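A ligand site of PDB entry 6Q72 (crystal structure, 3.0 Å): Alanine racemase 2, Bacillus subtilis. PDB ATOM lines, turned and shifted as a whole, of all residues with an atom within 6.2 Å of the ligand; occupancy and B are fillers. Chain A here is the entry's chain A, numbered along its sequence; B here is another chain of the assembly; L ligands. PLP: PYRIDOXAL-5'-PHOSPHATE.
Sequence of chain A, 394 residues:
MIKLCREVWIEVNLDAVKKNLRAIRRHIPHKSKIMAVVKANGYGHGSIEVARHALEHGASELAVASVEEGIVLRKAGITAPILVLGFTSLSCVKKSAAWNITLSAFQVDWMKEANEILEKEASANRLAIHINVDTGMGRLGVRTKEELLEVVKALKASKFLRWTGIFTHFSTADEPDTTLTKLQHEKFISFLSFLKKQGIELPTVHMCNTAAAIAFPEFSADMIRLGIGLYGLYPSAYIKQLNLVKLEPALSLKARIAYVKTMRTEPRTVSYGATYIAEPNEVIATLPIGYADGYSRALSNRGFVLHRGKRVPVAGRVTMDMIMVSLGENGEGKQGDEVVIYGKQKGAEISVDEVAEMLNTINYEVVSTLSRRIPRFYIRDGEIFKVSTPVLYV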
ATOM      1  N   VAL A  37     -15.911  32.730 -21.133  1.00  0.00           N
ATOM      2  CA  VAL A  37     -16.452  31.662 -20.289  1.00  0.00           C
ATOM      3  C   VAL A  37     -17.796  32.111 -19.709  1.00  0.00           C
ATOM      4  O   VAL A  37     -17.849  33.024 -18.904  1.00  0.00           O
ATOM      5  CB  VAL A  37     -15.487  31.285 -19.141  1.00  0.00           C
ATOM      6  CG1 VAL A  37     -16.049  30.053 -18.378  1.00  0.00           C
ATOM      7  CG2 VAL A  37     -14.120  30.945 -19.704  1.00  0.00           C
ATOM      8  N   LYS A  39     -20.157  29.938 -18.448  1.00  0.00           N
ATOM      9  CA  LYS A  39     -20.726  28.804 -17.751  1.00  0.00           C
ATOM     10  C   LYS A  39     -21.505  29.238 -16.530  1.00  0.00           C
ATOM     11  O   LYS A  39     -21.328  30.368 -16.086  1.00  0.00           O
ATOM     12  CB  LYS A  39     -19.626  27.842 -17.394  1.00  0.00           C
ATOM     13  CG  LYS A  39     -18.815  28.240 -16.166  1.00  0.00           C
ATOM     14  CD  LYS A  39     -17.620  27.320 -15.935  1.00  0.00           C
ATOM     15  CE  LYS A  39     -16.775  27.650 -14.702  1.00  0.00           C
ATOM     16  NZ  LYS A  39     -15.439  27.704 -15.265  1.00  0.00           N
ATOM     17  N   TYR A  43     -21.927  33.231 -15.236  1.00  0.00           N
ATOM     18  CA  TYR A  43     -21.547  33.569 -13.886  1.00  0.00           C
ATOM     19  C   TYR A  43     -22.664  34.344 -13.204  1.00  0.00           C
ATOM     20  O   TYR A  43     -22.408  35.311 -12.501  1.00  0.00           O
ATOM     21  CB  TYR A  43     -20.259  34.392 -13.861  1.00  0.00           C
ATOM     22  CG  TYR A  43     -18.964  33.658 -14.123  1.00  0.00           C
ATOM     23  CD1 TYR A  43     -18.865  32.632 -15.034  1.00  0.00           C
ATOM     24  CD2 TYR A  43     -17.809  34.030 -13.436  1.00  0.00           C
ATOM     25  CE1 TYR A  43     -17.643  31.985 -15.275  1.00  0.00           C
ATOM     26  CE2 TYR A  43     -16.610  33.406 -13.657  1.00  0.00           C
ATOM     27  CZ  TYR A  43     -16.521  32.396 -14.588  1.00  0.00           C
ATOM     28  OH  TYR A  43     -15.312  31.769 -14.787  1.00  0.00           O
ATOM     29  N   LEU A  85     -16.509  22.295 -20.706  1.00  0.00           N
ATOM     30  CA  LEU A  85     -15.254  22.163 -19.909  1.00  0.00           C
ATOM     31  C   LEU A  85     -15.205  20.922 -19.007  1.00  0.00           C
ATOM     32  O   LEU A  85     -14.104  20.431 -18.605  1.00  0.00           O
ATOM     33  CB  LEU A  85     -15.019  23.394 -19.031  1.00  0.00           C
ATOM     34  CG  LEU A  85     -14.817  24.704 -19.793  1.00  0.00           C
ATOM     35  CD1 LEU A  85     -14.894  25.875 -18.826  1.00  0.00           C
ATOM     36  CD2 LEU A  85     -13.499  24.704 -20.519  1.00  0.00           C
ATOM     37  N   ARG A 139      -8.355  17.722 -11.316  1.00  0.00           N
ATOM     38  CA  ARG A 139      -9.814  17.667 -11.446  1.00  0.00           C
ATOM     39  C   ARG A 139     -10.189  16.746 -12.600  1.00  0.00           C
ATOM     40  O   ARG A 139     -10.653  15.630 -12.387  1.00  0.00           O
ATOM     41  CB  ARG A 139     -10.381  19.085 -11.651  1.00  0.00           C
ATOM     42  CG  ARG A 139     -11.913  19.188 -11.704  1.00  0.00           C
ATOM     43  CD  ARG A 139     -12.317  20.636 -11.569  1.00  0.00           C
ATOM     44  NE  ARG A 139     -11.764  21.404 -12.682  1.00  0.00           N
ATOM     45  CZ  ARG A 139     -12.033  22.679 -12.906  1.00  0.00           C
ATOM     46  NH1 ARG A 139     -12.824  23.346 -12.082  1.00  0.00           N
ATOM     47  NH2 ARG A 139     -11.475  23.299 -13.954  1.00  0.00           N
ATOM     48  N   PHE A 167      -5.792  21.664 -23.927  1.00  0.00           N
ATOM     49  CA  PHE A 167      -5.700  22.625 -22.856  1.00  0.00           C
ATOM     50  C   PHE A 167      -5.306  22.037 -21.503  1.00  0.00           C
ATOM     51  O   PHE A 167      -5.341  20.833 -21.266  1.00  0.00           O
ATOM     52  CB  PHE A 167      -7.021  23.393 -22.729  1.00  0.00           C
ATOM     53  CG  PHE A 167      -8.202  22.602 -22.175  1.00  0.00           C
ATOM     54  CD1 PHE A 167      -9.007  21.835 -23.015  1.00  0.00           C
ATOM     55  CD2 PHE A 167      -8.549  22.692 -20.824  1.00  0.00           C
ATOM     56  CE1 PHE A 167     -10.150  21.150 -22.503  1.00  0.00           C
ATOM     57  CE2 PHE A 167      -9.669  21.989 -20.310  1.00  0.00           C
ATOM     58  CZ  PHE A 167     -10.460  21.223 -21.146  1.00  0.00           C
ATOM     59  N   THR A 168      -4.874  22.951 -20.641  1.00  0.00           N
ATOM     60  CA  THR A 168      -4.747  22.677 -19.227  1.00  0.00           C
ATOM     61  C   THR A 168      -5.249  23.846 -18.428  1.00  0.00           C
ATOM     62  O   THR A 168      -5.532  24.930 -18.947  1.00  0.00           O
ATOM     63  CB  THR A 168      -3.283  22.366 -18.815  1.00  0.00           C
ATOM     64  OG1 THR A 168      -3.294  21.799 -17.495  1.00  0.00           O
ATOM     65  CG2 THR A 168      -2.401  23.575 -18.842  1.00  0.00           C
ATOM     66  N   HIS A 169      -5.364  23.610 -17.140  1.00  0.00           N
ATOM     67  CA  HIS A 169      -5.842  24.524 -16.146  1.00  0.00           C
ATOM     68  C   HIS A 169      -4.875  24.731 -14.940  1.00  0.00           C
ATOM     69  O   HIS A 169      -4.407  23.824 -14.328  1.00  0.00           O
ATOM     70  CB  HIS A 169      -7.223  24.098 -15.692  1.00  0.00           C
ATOM     71  CG  HIS A 169      -8.093  25.232 -15.295  1.00  0.00           C
ATOM     72  ND1 HIS A 169      -8.621  26.230 -16.018  1.00  0.00           N
ATOM     73  CD2 HIS A 169      -8.495  25.455 -14.004  1.00  0.00           C
ATOM     74  CE1 HIS A 169      -9.322  27.028 -15.166  1.00  0.00           C
ATOM     75  NE2 HIS A 169      -9.257  26.527 -13.961  1.00  0.00           N
ATOM     76  N   CYS A 208      -4.585  29.719 -20.292  1.00  0.00           N
ATOM     77  CA  CYS A 208      -4.876  30.777 -19.390  1.00  0.00           C
ATOM     78  C   CYS A 208      -6.321  31.080 -19.012  1.00  0.00           C
ATOM     79  O   CYS A 208      -7.162  31.165 -19.832  1.00  0.00           O
ATOM     80  CB  CYS A 208      -4.298  32.115 -19.917  1.00  0.00           C
ATOM     81  SG  CYS A 208      -2.521  32.325 -19.961  1.00  0.00           S
ATOM     82  N   ASN A 209      -6.509  31.263 -17.739  1.00  0.00           N
ATOM     83  CA  ASN A 209      -7.685  31.763 -17.149  1.00  0.00           C
ATOM     84  C   ASN A 209      -7.450  33.281 -17.063  1.00  0.00           C
ATOM     85  O   ASN A 209      -6.491  33.757 -17.526  1.00  0.00           O
ATOM     86  CB  ASN A 209      -7.977  31.173 -15.757  1.00  0.00           C
ATOM     87  CG  ASN A 209      -6.720  31.010 -14.818  1.00  0.00           C
ATOM     88  OD1 ASN A 209      -5.662  31.577 -14.966  1.00  0.00           O
ATOM     89  ND2 ASN A 209      -6.908  30.174 -13.808  1.00  0.00           N
ATOM     90  N   THR A 210      -8.375  33.986 -16.442  1.00  0.00           N
ATOM     91  CA  THR A 210      -8.253  35.390 -16.249  1.00  0.00           C
ATOM     92  C   THR A 210      -6.924  35.713 -15.508  1.00  0.00           C
ATOM     93  O   THR A 210      -6.174  36.536 -15.973  1.00  0.00           O
ATOM     94  CB  THR A 210      -9.453  36.050 -15.517  1.00  0.00           C
ATOM     95  OG1 THR A 210     -10.680  35.846 -16.187  1.00  0.00           O
ATOM     96  CG2 THR A 210      -9.251  37.502 -15.368  1.00  0.00           C
ATOM     97  N   ALA A 211      -6.620  35.034 -14.418  1.00  0.00           N
ATOM     98  CA  ALA A 211      -5.419  35.333 -13.598  1.00  0.00           C
ATOM     99  C   ALA A 211      -4.152  35.257 -14.435  1.00  0.00           C
ATOM    100  O   ALA A 211      -3.382  36.216 -14.447  1.00  0.00           O
ATOM    101  CB  ALA A 211      -5.285  34.391 -12.382  1.00  0.00           C
ATOM    102  N   ARG A 225      -8.927  31.655 -21.879  1.00  0.00           N
ATOM    103  CA  ARG A 225     -10.292  31.472 -21.434  1.00  0.00           C
ATOM    104  C   ARG A 225     -10.610  32.569 -20.446  1.00  0.00           C
ATOM    105  O   ARG A 225     -10.178  32.524 -19.267  1.00  0.00           O
ATOM    106  CB  ARG A 225     -10.484  30.077 -20.844  1.00  0.00           C
ATOM    107  CG  ARG A 225     -10.174  28.952 -21.849  1.00  0.00           C
ATOM    108  CD  ARG A 225     -10.425  27.544 -21.277  1.00  0.00           C
ATOM    109  NE  ARG A 225      -9.768  27.291 -20.011  1.00  0.00           N
ATOM    110  CZ  ARG A 225      -8.533  26.796 -19.861  1.00  0.00           C
ATOM    111  NH1 ARG A 225      -7.788  26.515 -20.901  1.00  0.00           N
ATOM    112  NH2 ARG A 225      -8.050  26.593 -18.649  1.00  0.00           N
ATOM    113  N   LEU A 226     -11.366  33.549 -20.915  1.00  0.00           N
ATOM    114  CA  LEU A 226     -11.728  34.685 -20.108  1.00  0.00           C
ATOM    115  C   LEU A 226     -13.067  34.500 -19.374  1.00  0.00           C
ATOM    116  O   LEU A 226     -14.159  34.615 -19.977  1.00  0.00           O
ATOM    117  CB  LEU A 226     -11.794  35.958 -20.955  1.00  0.00           C
ATOM    118  CG  LEU A 226     -12.053  37.223 -20.139  1.00  0.00           C
ATOM    119  CD1 LEU A 226     -10.853  37.566 -19.195  1.00  0.00           C
ATOM    120  CD2 LEU A 226     -12.369  38.366 -21.075  1.00  0.00           C
ATOM    121  N   GLY A 227     -12.947  34.336 -18.055  1.00  0.00           N
ATOM    122  CA  GLY A 227     -14.078  34.169 -17.171  1.00  0.00           C
ATOM    123  C   GLY A 227     -14.371  35.393 -16.351  1.00  0.00           C
ATOM    124  O   GLY A 227     -14.963  36.365 -16.854  1.00  0.00           O
ATOM    125  N   ILE A 228     -13.935  35.358 -15.106  1.00  0.00           N
ATOM    126  CA  ILE A 228     -14.299  36.351 -14.098  1.00  0.00           C
ATOM    127  C   ILE A 228     -14.023  37.766 -14.601  1.00  0.00           C
ATOM    128  O   ILE A 228     -14.821  38.685 -14.367  1.00  0.00           O
ATOM    129  CB  ILE A 228     -13.543  36.070 -12.752  1.00  0.00           C
ATOM    130  CG1 ILE A 228     -14.134  36.891 -11.605  1.00  0.00           C
ATOM    131  CG2 ILE A 228     -12.018  36.326 -12.858  1.00  0.00           C
ATOM    132  CD1 ILE A 228     -15.573  36.591 -11.255  1.00  0.00           C
ATOM    133  N   GLY A 229     -12.925  37.922 -15.327  1.00  0.00           N
ATOM    134  CA  GLY A 229     -12.537  39.218 -15.847  1.00  0.00           C
ATOM    135  C   GLY A 229     -13.521  39.812 -16.839  1.00  0.00           C
ATOM    136  O   GLY A 229     -13.656  41.027 -16.938  1.00  0.00           O
ATOM    137  N   PRO A 235      -9.760  37.845 -10.329  1.00  0.00           N
ATOM    138  CA  PRO A 235      -9.690  36.520  -9.723  1.00  0.00           C
ATOM    139  C   PRO A 235      -9.122  36.509  -8.293  1.00  0.00           C
ATOM    140  O   PRO A 235      -9.318  35.533  -7.618  1.00  0.00           O
ATOM    141  CB  PRO A 235      -8.781  35.732 -10.669  1.00  0.00           C
ATOM    142  CG  PRO A 235      -7.961  36.761 -11.390  1.00  0.00           C
ATOM    143  CD  PRO A 235      -8.850  37.997 -11.481  1.00  0.00           C
ATOM    144  N   TYR A 364     -16.588  35.099  -7.348  1.00  0.00           N
ATOM    145  CA  TYR A 364     -17.183  34.077  -8.220  1.00  0.00           C
ATOM    146  C   TYR A 364     -18.490  33.485  -7.624  1.00  0.00           C
ATOM    147  O   TYR A 364     -19.506  33.301  -8.322  1.00  0.00           O
ATOM    148  CB  TYR A 364     -16.242  32.889  -8.452  1.00  0.00           C
ATOM    149  CG  TYR A 364     -14.936  33.097  -9.180  1.00  0.00           C
ATOM    150  CD1 TYR A 364     -13.873  33.733  -8.545  1.00  0.00           C
ATOM    151  CD2 TYR A 364     -14.730  32.537 -10.441  1.00  0.00           C
ATOM    152  CE1 TYR A 364     -12.655  33.844  -9.156  1.00  0.00           C
ATOM    153  CE2 TYR A 364     -13.488  32.673 -11.094  1.00  0.00           C
ATOM    154  CZ  TYR A 364     -12.460  33.350 -10.428  1.00  0.00           C
ATOM    155  OH  TYR A 364     -11.207  33.512 -10.968  1.00  0.00           O
ATOM    156  N   TYR B 272      -8.254  24.214  -6.490  1.00  0.00           N
ATOM    157  CA  TYR B 272      -7.694  25.554  -6.318  1.00  0.00           C
ATOM    158  C   TYR B 272      -6.973  25.743  -4.957  1.00  0.00           C
ATOM    159  O   TYR B 272      -7.327  25.100  -3.947  1.00  0.00           O
ATOM    160  CB  TYR B 272      -8.809  26.597  -6.484  1.00  0.00           C
ATOM    161  CG  TYR B 272      -9.340  26.769  -7.892  1.00  0.00           C
ATOM    162  CD1 TYR B 272      -8.496  27.123  -8.924  1.00  0.00           C
ATOM    163  CD2 TYR B 272     -10.688  26.581  -8.169  1.00  0.00           C
ATOM    164  CE1 TYR B 272      -8.967  27.303 -10.201  1.00  0.00           C
ATOM    165  CE2 TYR B 272     -11.186  26.747  -9.424  1.00  0.00           C
ATOM    166  CZ  TYR B 272     -10.312  27.121 -10.465  1.00  0.00           C
ATOM    167  OH  TYR B 272     -10.738  27.309 -11.750  1.00  0.00           O
ATOM    168  N   MET B 320     -16.551  25.842  -9.096  1.00  0.00           N
ATOM    169  CA  MET B 320     -17.839  26.406  -9.486  1.00  0.00           C
ATOM    170  C   MET B 320     -18.818  25.301  -9.934  1.00  0.00           C
ATOM    171  O   MET B 320     -20.004  25.360  -9.616  1.00  0.00           O
ATOM    172  CB  MET B 320     -17.697  27.432 -10.585  1.00  0.00           C
ATOM    173  CG  MET B 320     -19.045  28.087 -10.919  1.00  0.00           C
ATOM    174  SD  MET B 320     -18.911  29.392 -12.172  1.00  0.00           S
ATOM    175  CE  MET B 320     -17.801  30.572 -11.330  1.00  0.00           C
ATOM    176  N   ASP B 321     -18.294  24.283 -10.623  1.00  0.00           N
ATOM    177  CA  ASP B 321     -19.115  23.201 -11.206  1.00  0.00           C
ATOM    178  C   ASP B 321     -18.735  21.797 -10.771  1.00  0.00           C
ATOM    179  O   ASP B 321     -19.415  20.846 -11.155  1.00  0.00           O
ATOM    180  CB  ASP B 321     -19.028  23.252 -12.707  1.00  0.00           C
ATOM    181  CG  ASP B 321     -19.180  24.641 -13.247  1.00  0.00           C
ATOM    182  OD1 ASP B 321     -20.180  25.287 -12.899  1.00  0.00           O
ATOM    183  OD2 ASP B 321     -18.268  25.093 -13.990  1.00  0.00           O
ATOM    184  N   MET B 322     -17.662  21.678  -9.984  1.00  0.00           N
ATOM    185  CA  MET B 322     -17.126  20.345  -9.664  1.00  0.00           C
ATOM    186  C   MET B 322     -16.529  20.286  -8.269  1.00  0.00           C
ATOM    187  O   MET B 322     -16.091  21.289  -7.712  1.00  0.00           O
ATOM    188  CB  MET B 322     -16.042  19.942 -10.687  1.00  0.00           C
ATOM    189  CG  MET B 322     -16.580  19.456 -12.023  1.00  0.00           C
ATOM    190  SD  MET B 322     -15.258  18.923 -13.150  1.00  0.00           S
ATOM    191  CE  MET B 322     -14.924  20.488 -13.975  1.00  0.00           C
HETATM  192  N1  PLP L   1     -10.967  27.810 -17.385  1.00  0.00           N
HETATM  193  C2  PLP L   1     -11.590  26.693 -16.960  1.00  0.00           C
HETATM  194  C2A PLP L   1     -11.117  25.318 -17.378  1.00  0.00           C
HETATM  195  C3  PLP L   1     -12.740  26.806 -16.076  1.00  0.00           C
HETATM  196  O3  PLP L   1     -13.345  25.694 -15.666  1.00  0.00           O
HETATM  197  C4  PLP L   1     -13.193  28.125 -15.654  1.00  0.00           C
HETATM  198  C4A PLP L   1     -14.395  28.239 -14.772  1.00  0.00           C
HETATM  199  C5  PLP L   1     -12.432  29.275 -16.196  1.00  0.00           C
HETATM  200  C6  PLP L   1     -11.357  29.041 -17.029  1.00  0.00           C
HETATM  201  C5A PLP L   1     -12.753  30.701 -15.866  1.00  0.00           C
HETATM  202  O4P PLP L   1     -11.567  31.316 -15.384  1.00  0.00           O
HETATM  203  P   PLP L   1     -11.631  32.550 -14.432  1.00  0.00           P
HETATM  204  O1P PLP L   1     -11.247  32.010 -13.114  1.00  0.00           O
HETATM  205  O2P PLP L   1     -13.030  33.008 -14.504  1.00  0.00           O
HETATM  206  O3P PLP L   1     -10.654  33.463 -15.064  1.00  0.00           O
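The side-chain hydroxyl of Thr 210 is in hydrogen-bond range of the backbone NH of Ile 228 (3.5 Å).
N of Gly 227 sits at hydrogen-bond distance from OG1 of Thr 210.
OG1 of Thr 210 is in hydrogen-bond range of N of Gly 229 (3.2 Å).
The guanidinium group (NH2) of Arg 225 lies within hydrogen-bond range of a ring nitrogen (ND1) of His 169 (2.7 Å).
The side-chain hydroxyl (OH) of Tyr 272 of chain B sits at hydrogen-bond distance from a ring nitrogen (NE2) of His 169 (2.8 Å).
The backbone carbonyl oxygen (O) of Cys 208 lies within hydrogen-bond range of the backbone NH (N) of Arg 225 (2.7 Å).
The guanidinium group (NH2) of Arg 225 is in hydrogen-bond range of the backbone carbonyl oxygen (O) of Thr 168.
Merely in contact with the ligand: Gly 227 (3.1 Å), Leu 85 (3.5 Å) and Asn 209 (3.6 Å).
11 residues have an atom within 4 Å of the ligand: Lys 39, Tyr 43, Leu 85, Arg 139, His 169, Asn 209, Thr 210, Arg 225, Gly 227, Ile 228 and Tyr 364.
The nearest printed residue that does not touch the ligand is Val 37 (4.1 Å).
NZ of Lys 39 is covalently linked to C4A of the ligand (1.3 Å).
O2P of the ligand is in hydrogen-bond range of N of Ile 228 (2.6 Å).
An oxygen (O2P) of the ligand is in hydrogen-bond range of the side-chain hydroxyl (OH) of Tyr 43 (2.6 Å).
O1P of the ligand lies within hydrogen-bond range of OH of Tyr 364, 2.6 Å away.
The backbone NH of Thr 210 lies within hydrogen-bond range of an oxygen (O3P) of the ligand, 2.7 Å away.
The side-chain hydroxyl (OG1) of Thr 210 lies within hydrogen-bond range of an oxygen (O3P) of the ligand (2.6 Å).
ND1 of His 169 sits close to N1 of the ligand (3.1 Å).
NE of Arg 225 sits at hydrogen-bond distance from N1 of the ligand (2.9 Å).
The guanidinium group of Arg 139 lies within hydrogen-bond range of an oxygen (O3) of the ligand (3.5 Å).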
